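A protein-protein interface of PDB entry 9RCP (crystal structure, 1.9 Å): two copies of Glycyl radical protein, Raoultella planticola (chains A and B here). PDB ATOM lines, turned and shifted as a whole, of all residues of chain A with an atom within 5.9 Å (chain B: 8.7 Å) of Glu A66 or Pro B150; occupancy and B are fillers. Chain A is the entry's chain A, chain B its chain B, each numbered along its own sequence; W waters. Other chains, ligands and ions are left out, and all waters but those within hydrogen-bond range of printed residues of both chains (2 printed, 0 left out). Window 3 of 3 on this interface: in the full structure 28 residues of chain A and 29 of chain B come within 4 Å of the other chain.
The backbone carbonyl oxygen of Gln A67 lies within hydrogen-bond range of the side-chain hydroxyl of Ser B160 (3.2 Å). The backbone carbonyl oxygen (O) of Glu A66 lies close to the backbone carbonyl oxygen (O) of Gly B151 (3.1 Å). NH2 of Arg B539 lies within hydrogen-bond range of O of Glu A66 (2.7 Å). N of Gln A67 lies close to O of Gly B151 (3.2 Å).
The guanidinium group (NH1) of Arg B539 is in hydrogen-bond range of the backbone carbonyl oxygen (O) of Thr B153. NZ of Lys A152 is in salt-bridge range of OE2 of Glu A66. O of Gly B151 is in hydrogen-bond range of NH1 of Arg B539, 2.9 Å away. The backbone carbonyl oxygen of Gly B151 sits at hydrogen-bond distance from the side-chain hydroxyl of Ser B156, 3.2 Å away. OG of Ser B160 sits at hydrogen-bond distance from O of Ser B156 (3.0 Å). O of Glu A66 sits at hydrogen-bond distance from NH2 of Arg A73 (3.3 Å).
Pro B150 touches Glu A66 (O to CB, 3.9 Å). OE1 of Glu A66 touches CE of Lys B152, 3.9 Å away. OG of Ser B156 touches CB of Gln A67, at 3.6 Å. Gln A67 touches Leu B157 (O to CA, 3.3 Å). CD1 of Leu B157 touches C of Leu A68, at 3.9 Å. Leu A68 touches Ser B160. CE of Lys A152 touches CD of Glu B66, at 3.9 Å. Lys B152 touches Lys A152.
Glu A66 touches just these residues of chain B: Pro B150 (3.9 Å), Gly B151 (3.1 Å), Lys B152 (3.9 Å) and Arg B539 (2.7 Å). Of the printed residues of chain B, Gln A67 touches Gly B151 (3.1 Å), Ser B156 (3.6 Å), Leu B157 (3.3 Å) and Ser B160 (3.2 Å). Pro B150 touches just one residue of chain A: Glu A66 (3.9 Å). Of the printed residues of chain A, Ser B160 touches Gln A67 (3.2 Å) and Leu A68 (3.7 Å). The nearest printed residue of chain A that does not touch Ser B156 is Glu A66 (5.7 Å).
Hydrophobic or aromatic side chains of chain A that line the printed part of chain B: Leu A68. Of the 20 printed residues of chain B, 8 touch a printed residue of chain A. Printed residues of chain B that touch a printed residue of chain A: Glu B66, Pro B150, Gly B151, Lys B152, Ser B156, Leu B157, Ser B160 and Arg B539. Hydrophobic or aromatic side chains of chain B that line the printed part of chain A: Leu B157.
Glu A66 touches Lys B152, and with the chains exchanged Lys A152 touches Glu B66. Lys B152 touches its own counterpart, Lys A152. Positions printed for both chains: 66, 148 and 152. Of the 12 pairs that touch across the chains among the printed residues, 3 have their exchanged pair printed and touching as well.
Water W1 lies within hydrogen-bond range of O of Glu A66 and NH2 of Arg B539. Water W2 lies within hydrogen-bond range of the backbone carbonyl oxygen (O) of Leu A68, the guanidinium group (NH1) of Arg A73 and the guanidinium group (NH2) of Arg B539.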
ATOM      1  N   ALA A  61     -17.693  11.888 -15.462  1.00  0.00           N
ATOM      2  CA  ALA A  61     -18.397  12.836 -16.324  1.00  0.00           C
ATOM      3  C   ALA A  61     -17.842  12.825 -17.747  1.00  0.00           C
ATOM      4  O   ALA A  61     -18.606  12.902 -18.715  1.00  0.00           O
ATOM      5  CB  ALA A  61     -18.328  14.244 -15.734  1.00  0.00           C
ATOM      6  N   TYR A  62     -16.516  12.725 -17.902  1.00  0.00           N
ATOM      7  CA  TYR A  62     -15.941  12.615 -19.245  1.00  0.00           C
ATOM      8  C   TYR A  62     -16.392  11.332 -19.938  1.00  0.00           C
ATOM      9  O   TYR A  62     -16.820  11.364 -21.097  1.00  0.00           O
ATOM     10  CB  TYR A  62     -14.406  12.676 -19.224  1.00  0.00           C
ATOM     11  CG  TYR A  62     -13.797  14.075 -19.140  1.00  0.00           C
ATOM     12  CD1 TYR A  62     -13.761  14.784 -17.948  1.00  0.00           C
ATOM     13  CD2 TYR A  62     -13.286  14.695 -20.283  1.00  0.00           C
ATOM     14  CE1 TYR A  62     -13.190  16.056 -17.877  1.00  0.00           C
ATOM     15  CE2 TYR A  62     -12.728  15.983 -20.228  1.00  0.00           C
ATOM     16  CZ  TYR A  62     -12.683  16.657 -19.020  1.00  0.00           C
ATOM     17  OH  TYR A  62     -12.157  17.932 -18.951  1.00  0.00           O
ATOM     18  N   LYS A  63     -16.284  10.189 -19.245  1.00  0.00           N
ATOM     19  CA  LYS A  63     -16.670   8.904 -19.826  1.00  0.00           C
ATOM     20  C   LYS A  63     -18.101   8.927 -20.333  1.00  0.00           C
ATOM     21  O   LYS A  63     -18.410   8.345 -21.381  1.00  0.00           O
ATOM     22  CB  LYS A  63     -16.536   7.782 -18.789  1.00  0.00           C
ATOM     23  CG  LYS A  63     -15.133   7.278 -18.494  1.00  0.00           C
ATOM     24  CD  LYS A  63     -15.167   6.221 -17.385  1.00  0.00           C
ATOM     25  CE  LYS A  63     -13.778   5.673 -17.062  1.00  0.00           C
ATOM     26  NZ  LYS A  63     -13.768   4.863 -15.803  1.00  0.00           N
ATOM     27  N   GLU A  64     -18.995   9.565 -19.576  1.00  0.00           N
ATOM     28  CA  GLU A  64     -20.429   9.591 -19.847  1.00  0.00           C
ATOM     29  C   GLU A  64     -20.815  10.540 -20.969  1.00  0.00           C
ATOM     30  O   GLU A  64     -21.973  10.526 -21.406  1.00  0.00           O
ATOM     31  CB  GLU A  64     -21.172   9.997 -18.571  1.00  0.00           C
ATOM     32  CG  GLU A  64     -21.387   8.839 -17.626  1.00  0.00           C
ATOM     33  CD  GLU A  64     -21.614   9.276 -16.198  1.00  0.00           C
ATOM     34  OE1 GLU A  64     -21.160   8.539 -15.302  1.00  0.00           O
ATOM     35  OE2 GLU A  64     -22.215  10.350 -15.976  1.00  0.00           O
ATOM     36  N   ASN A  65     -19.897  11.379 -21.430  1.00  0.00           N
ATOM     37  CA  ASN A  65     -20.271  12.499 -22.278  1.00  0.00           C
ATOM     38  C   ASN A  65     -19.274  12.665 -23.422  1.00  0.00           C
ATOM     39  O   ASN A  65     -18.948  13.786 -23.818  1.00  0.00           O
ATOM     40  CB  ASN A  65     -20.379  13.766 -21.432  1.00  0.00           C
ATOM     41  CG  ASN A  65     -21.548  13.703 -20.439  1.00  0.00           C
ATOM     42  OD1 ASN A  65     -22.720  13.779 -20.822  1.00  0.00           O
ATOM     43  ND2 ASN A  65     -21.224  13.490 -19.164  1.00  0.00           N
ATOM     44  N   GLU A  66     -18.798  11.545 -23.984  1.00  0.00           N
ATOM     45  CA  GLU A  66     -17.846  11.596 -25.097  1.00  0.00           C
ATOM     46  C   GLU A  66     -18.386  12.393 -26.286  1.00  0.00           C
ATOM     47  O   GLU A  66     -17.609  13.025 -27.010  1.00  0.00           O
ATOM     48  CB  GLU A  66     -17.507  10.176 -25.567  1.00  0.00           C
ATOM     49  CG  GLU A  66     -16.777   9.241 -24.576  1.00  0.00           C
ATOM     50  CD  GLU A  66     -15.295   9.573 -24.349  1.00  0.00           C
ATOM     51  OE1 GLU A  66     -14.726  10.415 -25.062  1.00  0.00           O
ATOM     52  OE2 GLU A  66     -14.682   8.941 -23.469  1.00  0.00           O
ATOM     53  N   GLN A  67     -19.702  12.338 -26.532  1.00  0.00           N
ATOM     54  CA  GLN A  67     -20.306  12.872 -27.753  1.00  0.00           C
ATOM     55  C   GLN A  67     -20.483  14.384 -27.739  1.00  0.00           C
ATOM     56  O   GLN A  67     -20.862  14.953 -28.768  1.00  0.00           O
ATOM     57  CB  GLN A  67     -21.687  12.225 -27.999  1.00  0.00           C
ATOM     58  CG  GLN A  67     -22.803  12.827 -27.169  1.00  0.00           C
ATOM     59  CD  GLN A  67     -22.911  12.220 -25.772  1.00  0.00           C
ATOM     60  OE1 GLN A  67     -22.037  11.471 -25.329  1.00  0.00           O
ATOM     61  NE2 GLN A  67     -23.991  12.536 -25.081  1.00  0.00           N
ATOM     62  N   LEU A  68     -20.242  15.043 -26.612  1.00  0.00           N
ATOM     63  CA  LEU A  68     -20.643  16.436 -26.535  1.00  0.00           C
ATOM     64  C   LEU A  68     -19.524  17.356 -27.007  1.00  0.00           C
ATOM     65  O   LEU A  68     -18.343  17.007 -26.908  1.00  0.00           O
ATOM     66  CB  LEU A  68     -21.001  16.801 -25.098  1.00  0.00           C
ATOM     67  CG  LEU A  68     -22.246  16.169 -24.494  1.00  0.00           C
ATOM     68  CD1 LEU A  68     -22.391  16.674 -23.064  1.00  0.00           C
ATOM     69  CD2 LEU A  68     -23.476  16.507 -25.329  1.00  0.00           C
ATOM     70  N   ARG A  73     -19.398  19.342 -22.375  1.00  0.00           N
ATOM     71  CA  ARG A  73     -18.781  18.260 -21.583  1.00  0.00           C
ATOM     72  C   ARG A  73     -18.296  18.878 -20.261  1.00  0.00           C
ATOM     73  O   ARG A  73     -18.522  18.297 -19.230  1.00  0.00           O
ATOM     74  CB  ARG A  73     -17.650  17.603 -22.370  1.00  0.00           C
ATOM     75  CG  ARG A  73     -16.991  16.466 -21.619  1.00  0.00           C
ATOM     76  CD  ARG A  73     -16.236  15.452 -22.444  1.00  0.00           C
ATOM     77  NE  ARG A  73     -15.436  16.161 -23.408  1.00  0.00           N
ATOM     78  CZ  ARG A  73     -15.735  16.205 -24.667  1.00  0.00           C
ATOM     79  NH1 ARG A  73     -14.969  16.884 -25.492  1.00  0.00           N
ATOM     80  NH2 ARG A  73     -16.780  15.544 -25.086  1.00  0.00           N
ATOM     81  N   TYR A 148      -8.433   6.016 -17.700  1.00  0.00           N
ATOM     82  CA  TYR A 148      -9.187   6.699 -18.743  1.00  0.00           C
ATOM     83  C   TYR A 148      -8.324   7.668 -19.545  1.00  0.00           C
ATOM     84  O   TYR A 148      -8.568   7.880 -20.735  1.00  0.00           O
ATOM     85  CB  TYR A 148     -10.361   7.452 -18.114  1.00  0.00           C
ATOM     86  CG  TYR A 148     -11.108   8.289 -19.110  1.00  0.00           C
ATOM     87  CD1 TYR A 148     -12.021   7.706 -19.996  1.00  0.00           C
ATOM     88  CD2 TYR A 148     -10.882   9.649 -19.204  1.00  0.00           C
ATOM     89  CE1 TYR A 148     -12.715   8.474 -20.923  1.00  0.00           C
ATOM     90  CE2 TYR A 148     -11.581  10.425 -20.128  1.00  0.00           C
ATOM     91  CZ  TYR A 148     -12.490   9.835 -20.979  1.00  0.00           C
ATOM     92  OH  TYR A 148     -13.160  10.601 -21.908  1.00  0.00           O
ATOM     93  N   LYS A 152      -5.643  12.008 -23.488  1.00  0.00           N
ATOM     94  CA  LYS A 152      -6.871  12.802 -23.456  1.00  0.00           C
ATOM     95  C   LYS A 152      -6.745  14.060 -22.604  1.00  0.00           C
ATOM     96  O   LYS A 152      -7.719  14.805 -22.461  1.00  0.00           O
ATOM     97  CB  LYS A 152      -8.045  11.951 -22.948  1.00  0.00           C
ATOM     98  CG  LYS A 152      -8.367  10.767 -23.860  1.00  0.00           C
ATOM     99  CD  LYS A 152      -9.502   9.918 -23.324  1.00  0.00           C
ATOM    100  CE  LYS A 152      -9.807   8.759 -24.278  1.00  0.00           C
ATOM    101  NZ  LYS A 152     -10.860   7.855 -23.737  1.00  0.00           N
ATOM    102  N   GLU B  66      -4.696   9.279 -29.547  1.00  0.00           N
ATOM    103  CA  GLU B  66      -5.644  10.134 -28.834  1.00  0.00           C
ATOM    104  C   GLU B  66      -5.122  11.555 -28.662  1.00  0.00           C
ATOM    105  O   GLU B  66      -5.911  12.502 -28.637  1.00  0.00           O
ATOM    106  CB  GLU B  66      -5.937   9.547 -27.452  1.00  0.00           C
ATOM    107  CG  GLU B  66      -6.640   8.185 -27.385  1.00  0.00           C
ATOM    108  CD  GLU B  66      -8.102   8.230 -27.797  1.00  0.00           C
ATOM    109  OE1 GLU B  66      -8.630   9.332 -28.021  1.00  0.00           O
ATOM    110  OE2 GLU B  66      -8.739   7.164 -27.848  1.00  0.00           O
ATOM    111  N   PRO B 110     -16.324   3.433 -39.328  1.00  0.00           N
ATOM    112  CA  PRO B 110     -17.038   3.684 -38.068  1.00  0.00           C
ATOM    113  C   PRO B 110     -16.800   5.066 -37.491  1.00  0.00           C
ATOM    114  O   PRO B 110     -17.523   5.447 -36.565  1.00  0.00           O
ATOM    115  CB  PRO B 110     -16.479   2.604 -37.126  1.00  0.00           C
ATOM    116  CG  PRO B 110     -15.054   2.440 -37.602  1.00  0.00           C
ATOM    117  CD  PRO B 110     -15.115   2.613 -39.127  1.00  0.00           C
ATOM    118  N   TYR B 114     -21.507   3.785 -36.620  1.00  0.00           N
ATOM    119  CA  TYR B 114     -21.297   2.338 -36.599  1.00  0.00           C
ATOM    120  C   TYR B 114     -22.488   1.528 -36.103  1.00  0.00           C
ATOM    121  O   TYR B 114     -22.578   0.347 -36.457  1.00  0.00           O
ATOM    122  CB  TYR B 114     -20.081   1.995 -35.713  1.00  0.00           C
ATOM    123  CG  TYR B 114     -20.397   2.314 -34.274  1.00  0.00           C
ATOM    124  CD1 TYR B 114     -20.318   3.620 -33.811  1.00  0.00           C
ATOM    125  CD2 TYR B 114     -20.839   1.323 -33.390  1.00  0.00           C
ATOM    126  CE1 TYR B 114     -20.655   3.939 -32.513  1.00  0.00           C
ATOM    127  CE2 TYR B 114     -21.183   1.634 -32.089  1.00  0.00           C
ATOM    128  CZ  TYR B 114     -21.086   2.945 -31.660  1.00  0.00           C
ATOM    129  OH  TYR B 114     -21.415   3.285 -30.376  1.00  0.00           O
ATOM    130  N   ASP B 115     -23.386   2.084 -35.272  1.00  0.00           N
ATOM    131  CA  ASP B 115     -24.251   1.200 -34.492  1.00  0.00           C
ATOM    132  C   ASP B 115     -25.235   0.445 -35.378  1.00  0.00           C
ATOM    133  O   ASP B 115     -25.589  -0.700 -35.067  1.00  0.00           O
ATOM    134  CB  ASP B 115     -24.977   1.960 -33.361  1.00  0.00           C
ATOM    135  CG  ASP B 115     -26.004   2.970 -33.853  1.00  0.00           C
ATOM    136  OD1 ASP B 115     -26.088   3.282 -35.063  1.00  0.00           O
ATOM    137  OD2 ASP B 115     -26.751   3.462 -32.982  1.00  0.00           O
ATOM    138  N   GLU B 118     -23.841  -3.058 -36.636  1.00  0.00           N
ATOM    139  CA  GLU B 118     -23.950  -4.175 -35.711  1.00  0.00           C
ATOM    140  C   GLU B 118     -25.412  -4.550 -35.472  1.00  0.00           C
ATOM    141  O   GLU B 118     -25.730  -5.737 -35.360  1.00  0.00           O
ATOM    142  CB  GLU B 118     -23.203  -3.818 -34.428  1.00  0.00           C
ATOM    143  CG  GLU B 118     -23.545  -4.564 -33.167  1.00  0.00           C
ATOM    144  CD  GLU B 118     -22.304  -4.692 -32.282  1.00  0.00           C
ATOM    145  OE1 GLU B 118     -22.044  -5.801 -31.779  1.00  0.00           O
ATOM    146  OE2 GLU B 118     -21.557  -3.700 -32.140  1.00  0.00           O
ATOM    147  N   HIS B 143     -17.574  -6.262 -34.223  1.00  0.00           N
ATOM    148  CA  HIS B 143     -18.081  -6.128 -32.851  1.00  0.00           C
ATOM    149  C   HIS B 143     -17.006  -5.607 -31.906  1.00  0.00           C
ATOM    150  O   HIS B 143     -17.265  -4.729 -31.073  1.00  0.00           O
ATOM    151  CB  HIS B 143     -18.601  -7.473 -32.336  1.00  0.00           C
ATOM    152  CG  HIS B 143     -18.931  -7.484 -30.870  1.00  0.00           C
ATOM    153  ND1 HIS B 143     -20.100  -6.959 -30.366  1.00  0.00           N
ATOM    154  CD2 HIS B 143     -18.245  -7.962 -29.802  1.00  0.00           C
ATOM    155  CE1 HIS B 143     -20.129  -7.118 -29.055  1.00  0.00           C
ATOM    156  NE2 HIS B 143     -19.014  -7.721 -28.686  1.00  0.00           N
ATOM    157  N   GLN B 144     -15.793  -6.145 -32.022  1.00  0.00           N
ATOM    158  CA  GLN B 144     -14.699  -5.744 -31.143  1.00  0.00           C
ATOM    159  C   GLN B 144     -14.245  -4.316 -31.434  1.00  0.00           C
ATOM    160  O   GLN B 144     -14.029  -3.523 -30.512  1.00  0.00           O
ATOM    161  CB  GLN B 144     -13.530  -6.718 -31.300  1.00  0.00           C
ATOM    162  CG  GLN B 144     -12.304  -6.350 -30.473  1.00  0.00           C
ATOM    163  CD  GLN B 144     -12.610  -6.314 -28.981  1.00  0.00           C
ATOM    164  OE1 GLN B 144     -13.466  -7.065 -28.488  1.00  0.00           O
ATOM    165  NE2 GLN B 144     -11.903  -5.451 -28.254  1.00  0.00           N
ATOM    166  N   ALA B 145     -14.083  -3.971 -32.715  1.00  0.00           N
ATOM    167  CA  ALA B 145     -13.669  -2.615 -33.064  1.00  0.00           C
ATOM    168  C   ALA B 145     -14.713  -1.588 -32.640  1.00  0.00           C
ATOM    169  O   ALA B 145     -14.363  -0.493 -32.179  1.00  0.00           O
ATOM    170  CB  ALA B 145     -13.402  -2.528 -34.565  1.00  0.00           C
ATOM    171  N   PHE B 146     -16.000  -1.928 -32.768  1.00  0.00           N
ATOM    172  CA  PHE B 146     -17.055  -0.993 -32.410  1.00  0.00           C
ATOM    173  C   PHE B 146     -17.050  -0.632 -30.927  1.00  0.00           C
ATOM    174  O   PHE B 146     -17.562   0.431 -30.565  1.00  0.00           O
ATOM    175  CB  PHE B 146     -18.437  -1.547 -32.794  1.00  0.00           C
ATOM    176  CG  PHE B 146     -18.669  -1.643 -34.283  1.00  0.00           C
ATOM    177  CD1 PHE B 146     -17.781  -1.071 -35.181  1.00  0.00           C
ATOM    178  CD2 PHE B 146     -19.783  -2.305 -34.782  1.00  0.00           C
ATOM    179  CE1 PHE B 146     -17.999  -1.150 -36.539  1.00  0.00           C
ATOM    180  CE2 PHE B 146     -20.003  -2.391 -36.146  1.00  0.00           C
ATOM    181  CZ  PHE B 146     -19.113  -1.815 -37.028  1.00  0.00           C
ATOM    182  N   LYS B 147     -16.483  -1.475 -30.060  1.00  0.00           N
ATOM    183  CA  LYS B 147     -16.409  -1.126 -28.643  1.00  0.00           C
ATOM    184  C   LYS B 147     -15.684   0.194 -28.398  1.00  0.00           C
ATOM    185  O   LYS B 147     -15.930   0.839 -27.374  1.00  0.00           O
ATOM    186  CB  LYS B 147     -15.716  -2.238 -27.853  1.00  0.00           C
ATOM    187  CG  LYS B 147     -16.485  -3.538 -27.780  1.00  0.00           C
ATOM    188  CD  LYS B 147     -15.695  -4.583 -26.991  1.00  0.00           C
ATOM    189  CE  LYS B 147     -16.393  -5.935 -26.979  1.00  0.00           C
ATOM    190  NZ  LYS B 147     -15.616  -6.973 -26.237  1.00  0.00           N
ATOM    191  N   TYR B 148     -14.823   0.627 -29.323  1.00  0.00           N
ATOM    192  CA  TYR B 148     -14.105   1.885 -29.141  1.00  0.00           C
ATOM    193  C   TYR B 148     -15.014   3.101 -29.325  1.00  0.00           C
ATOM    194  O   TYR B 148     -14.831   4.128 -28.657  1.00  0.00           O
ATOM    195  CB  TYR B 148     -12.940   1.952 -30.133  1.00  0.00           C
ATOM    196  CG  TYR B 148     -12.198   3.267 -30.104  1.00  0.00           C
ATOM    197  CD1 TYR B 148     -11.258   3.537 -29.109  1.00  0.00           C
ATOM    198  CD2 TYR B 148     -12.442   4.249 -31.057  1.00  0.00           C
ATOM    199  CE1 TYR B 148     -10.565   4.749 -29.072  1.00  0.00           C
ATOM    200  CE2 TYR B 148     -11.750   5.472 -31.022  1.00  0.00           C
ATOM    201  CZ  TYR B 148     -10.822   5.706 -30.027  1.00  0.00           C
ATOM    202  OH  TYR B 148     -10.144   6.899 -29.986  1.00  0.00           O
ATOM    203  N   TRP B 149     -15.961   3.021 -30.274  1.00  0.00           N
ATOM    204  CA  TRP B 149     -16.627   4.169 -30.902  1.00  0.00           C
ATOM    205  C   TRP B 149     -17.750   4.934 -30.188  1.00  0.00           C
ATOM    206  O   TRP B 149     -18.045   6.052 -30.636  1.00  0.00           O
ATOM    207  CB  TRP B 149     -17.081   3.756 -32.306  1.00  0.00           C
ATOM    208  CG  TRP B 149     -15.860   3.716 -33.172  1.00  0.00           C
ATOM    209  CD1 TRP B 149     -15.202   2.605 -33.617  1.00  0.00           C
ATOM    210  CD2 TRP B 149     -15.084   4.845 -33.603  1.00  0.00           C
ATOM    211  NE1 TRP B 149     -14.076   2.973 -34.341  1.00  0.00           N
ATOM    212  CE2 TRP B 149     -13.981   4.343 -34.336  1.00  0.00           C
ATOM    213  CE3 TRP B 149     -15.221   6.231 -33.456  1.00  0.00           C
ATOM    214  CZ2 TRP B 149     -13.030   5.180 -34.926  1.00  0.00           C
ATOM    215  CZ3 TRP B 149     -14.258   7.059 -34.036  1.00  0.00           C
ATOM    216  CH2 TRP B 149     -13.178   6.524 -34.760  1.00  0.00           C
ATOM    217  N   PRO B 150     -18.489   4.377 -29.160  1.00  0.00           N
ATOM    218  CA  PRO B 150     -19.609   5.143 -28.571  1.00  0.00           C
ATOM    219  C   PRO B 150     -19.295   6.604 -28.272  1.00  0.00           C
ATOM    220  O   PRO B 150     -18.367   6.899 -27.521  1.00  0.00           O
ATOM    221  CB  PRO B 150     -19.911   4.379 -27.274  1.00  0.00           C
ATOM    222  CG  PRO B 150     -19.516   2.989 -27.575  1.00  0.00           C
ATOM    223  CD  PRO B 150     -18.282   3.110 -28.435  1.00  0.00           C
ATOM    224  N   GLY B 151     -20.046   7.529 -28.866  1.00  0.00           N
ATOM    225  CA  GLY B 151     -19.845   8.936 -28.605  1.00  0.00           C
ATOM    226  C   GLY B 151     -18.624   9.571 -29.250  1.00  0.00           C
ATOM    227  O   GLY B 151     -18.406  10.769 -29.058  1.00  0.00           O
ATOM    228  N   LYS B 152     -17.819   8.824 -30.010  1.00  0.00           N
ATOM    229  CA  LYS B 152     -16.624   9.381 -30.636  1.00  0.00           C
ATOM    230  C   LYS B 152     -16.781   9.595 -32.135  1.00  0.00           C
ATOM    231  O   LYS B 152     -15.825  10.011 -32.799  1.00  0.00           O
ATOM    232  CB  LYS B 152     -15.411   8.480 -30.355  1.00  0.00           C
ATOM    233  CG  LYS B 152     -15.059   8.387 -28.882  1.00  0.00           C
ATOM    234  CD  LYS B 152     -13.857   7.474 -28.638  1.00  0.00           C
ATOM    235  CE  LYS B 152     -13.673   7.282 -27.126  1.00  0.00           C
ATOM    236  NZ  LYS B 152     -12.649   6.240 -26.812  1.00  0.00           N
ATOM    237  N   THR B 153     -17.959   9.320 -32.682  1.00  0.00           N
ATOM    238  CA  THR B 153     -18.258   9.504 -34.089  1.00  0.00           C
ATOM    239  C   THR B 153     -18.549  10.973 -34.399  1.00  0.00           C
ATOM    240  O   THR B 153     -18.888  11.767 -33.515  1.00  0.00           O
ATOM    241  CB  THR B 153     -19.468   8.652 -34.462  1.00  0.00           C
ATOM    242  OG1 THR B 153     -20.544   8.981 -33.570  1.00  0.00           O
ATOM    243  CG2 THR B 153     -19.120   7.162 -34.331  1.00  0.00           C
ATOM    244  N   SER B 156     -22.387  11.495 -33.677  1.00  0.00           N
ATOM    245  CA  SER B 156     -22.824  11.728 -32.300  1.00  0.00           C
ATOM    246  C   SER B 156     -22.564  13.173 -31.886  1.00  0.00           C
ATOM    247  O   SER B 156     -23.372  13.771 -31.171  1.00  0.00           O
ATOM    248  CB  SER B 156     -22.157  10.734 -31.343  1.00  0.00           C
ATOM    249  OG  SER B 156     -20.755  10.956 -31.229  1.00  0.00           O
ATOM    250  N   LEU B 157     -21.466  13.764 -32.358  1.00  0.00           N
ATOM    251  CA  LEU B 157     -21.216  15.177 -32.087  1.00  0.00           C
ATOM    252  C   LEU B 157     -22.194  16.070 -32.844  1.00  0.00           C
ATOM    253  O   LEU B 157     -22.723  17.032 -32.277  1.00  0.00           O
ATOM    254  CB  LEU B 157     -19.769  15.540 -32.439  1.00  0.00           C
ATOM    255  CG  LEU B 157     -19.319  16.996 -32.301  1.00  0.00           C
ATOM    256  CD1 LEU B 157     -19.391  17.470 -30.858  1.00  0.00           C
ATOM    257  CD2 LEU B 157     -17.898  17.177 -32.835  1.00  0.00           C
ATOM    258  N   SER B 160     -25.452  16.477 -31.168  1.00  0.00           N
ATOM    259  CA  SER B 160     -25.352  17.257 -29.936  1.00  0.00           C
ATOM    260  C   SER B 160     -25.429  18.755 -30.180  1.00  0.00           C
ATOM    261  O   SER B 160     -25.793  19.504 -29.260  1.00  0.00           O
ATOM    262  CB  SER B 160     -24.038  16.939 -29.202  1.00  0.00           C
ATOM    263  OG  SER B 160     -23.977  15.578 -28.843  1.00  0.00           O
ATOM    264  N   ARG B 539     -13.904  16.956 -35.828  1.00  0.00           N
ATOM    265  CA  ARG B 539     -13.452  15.590 -35.583  1.00  0.00           C
ATOM    266  C   ARG B 539     -12.860  14.883 -36.791  1.00  0.00           C
ATOM    267  O   ARG B 539     -12.153  13.891 -36.600  1.00  0.00           O
ATOM    268  CB  ARG B 539     -14.607  14.726 -35.049  1.00  0.00           C
ATOM    269  CG  ARG B 539     -14.952  15.038 -33.605  1.00  0.00           C
ATOM    270  CD  ARG B 539     -15.947  14.053 -32.991  1.00  0.00           C
ATOM    271  NE  ARG B 539     -16.049  14.307 -31.562  1.00  0.00           N
ATOM    272  CZ  ARG B 539     -16.776  13.597 -30.708  1.00  0.00           C
ATOM    273  NH1 ARG B 539     -17.500  12.573 -31.134  1.00  0.00           N
ATOM    274  NH2 ARG B 539     -16.777  13.926 -29.423  1.00  0.00           N
HETATM  275  O   HOH W   1     -15.018  12.384 -27.031  1.00  0.00           O
HETATM  276  O   HOH W   2     -15.933  16.687 -28.305  1.00  0.00           O
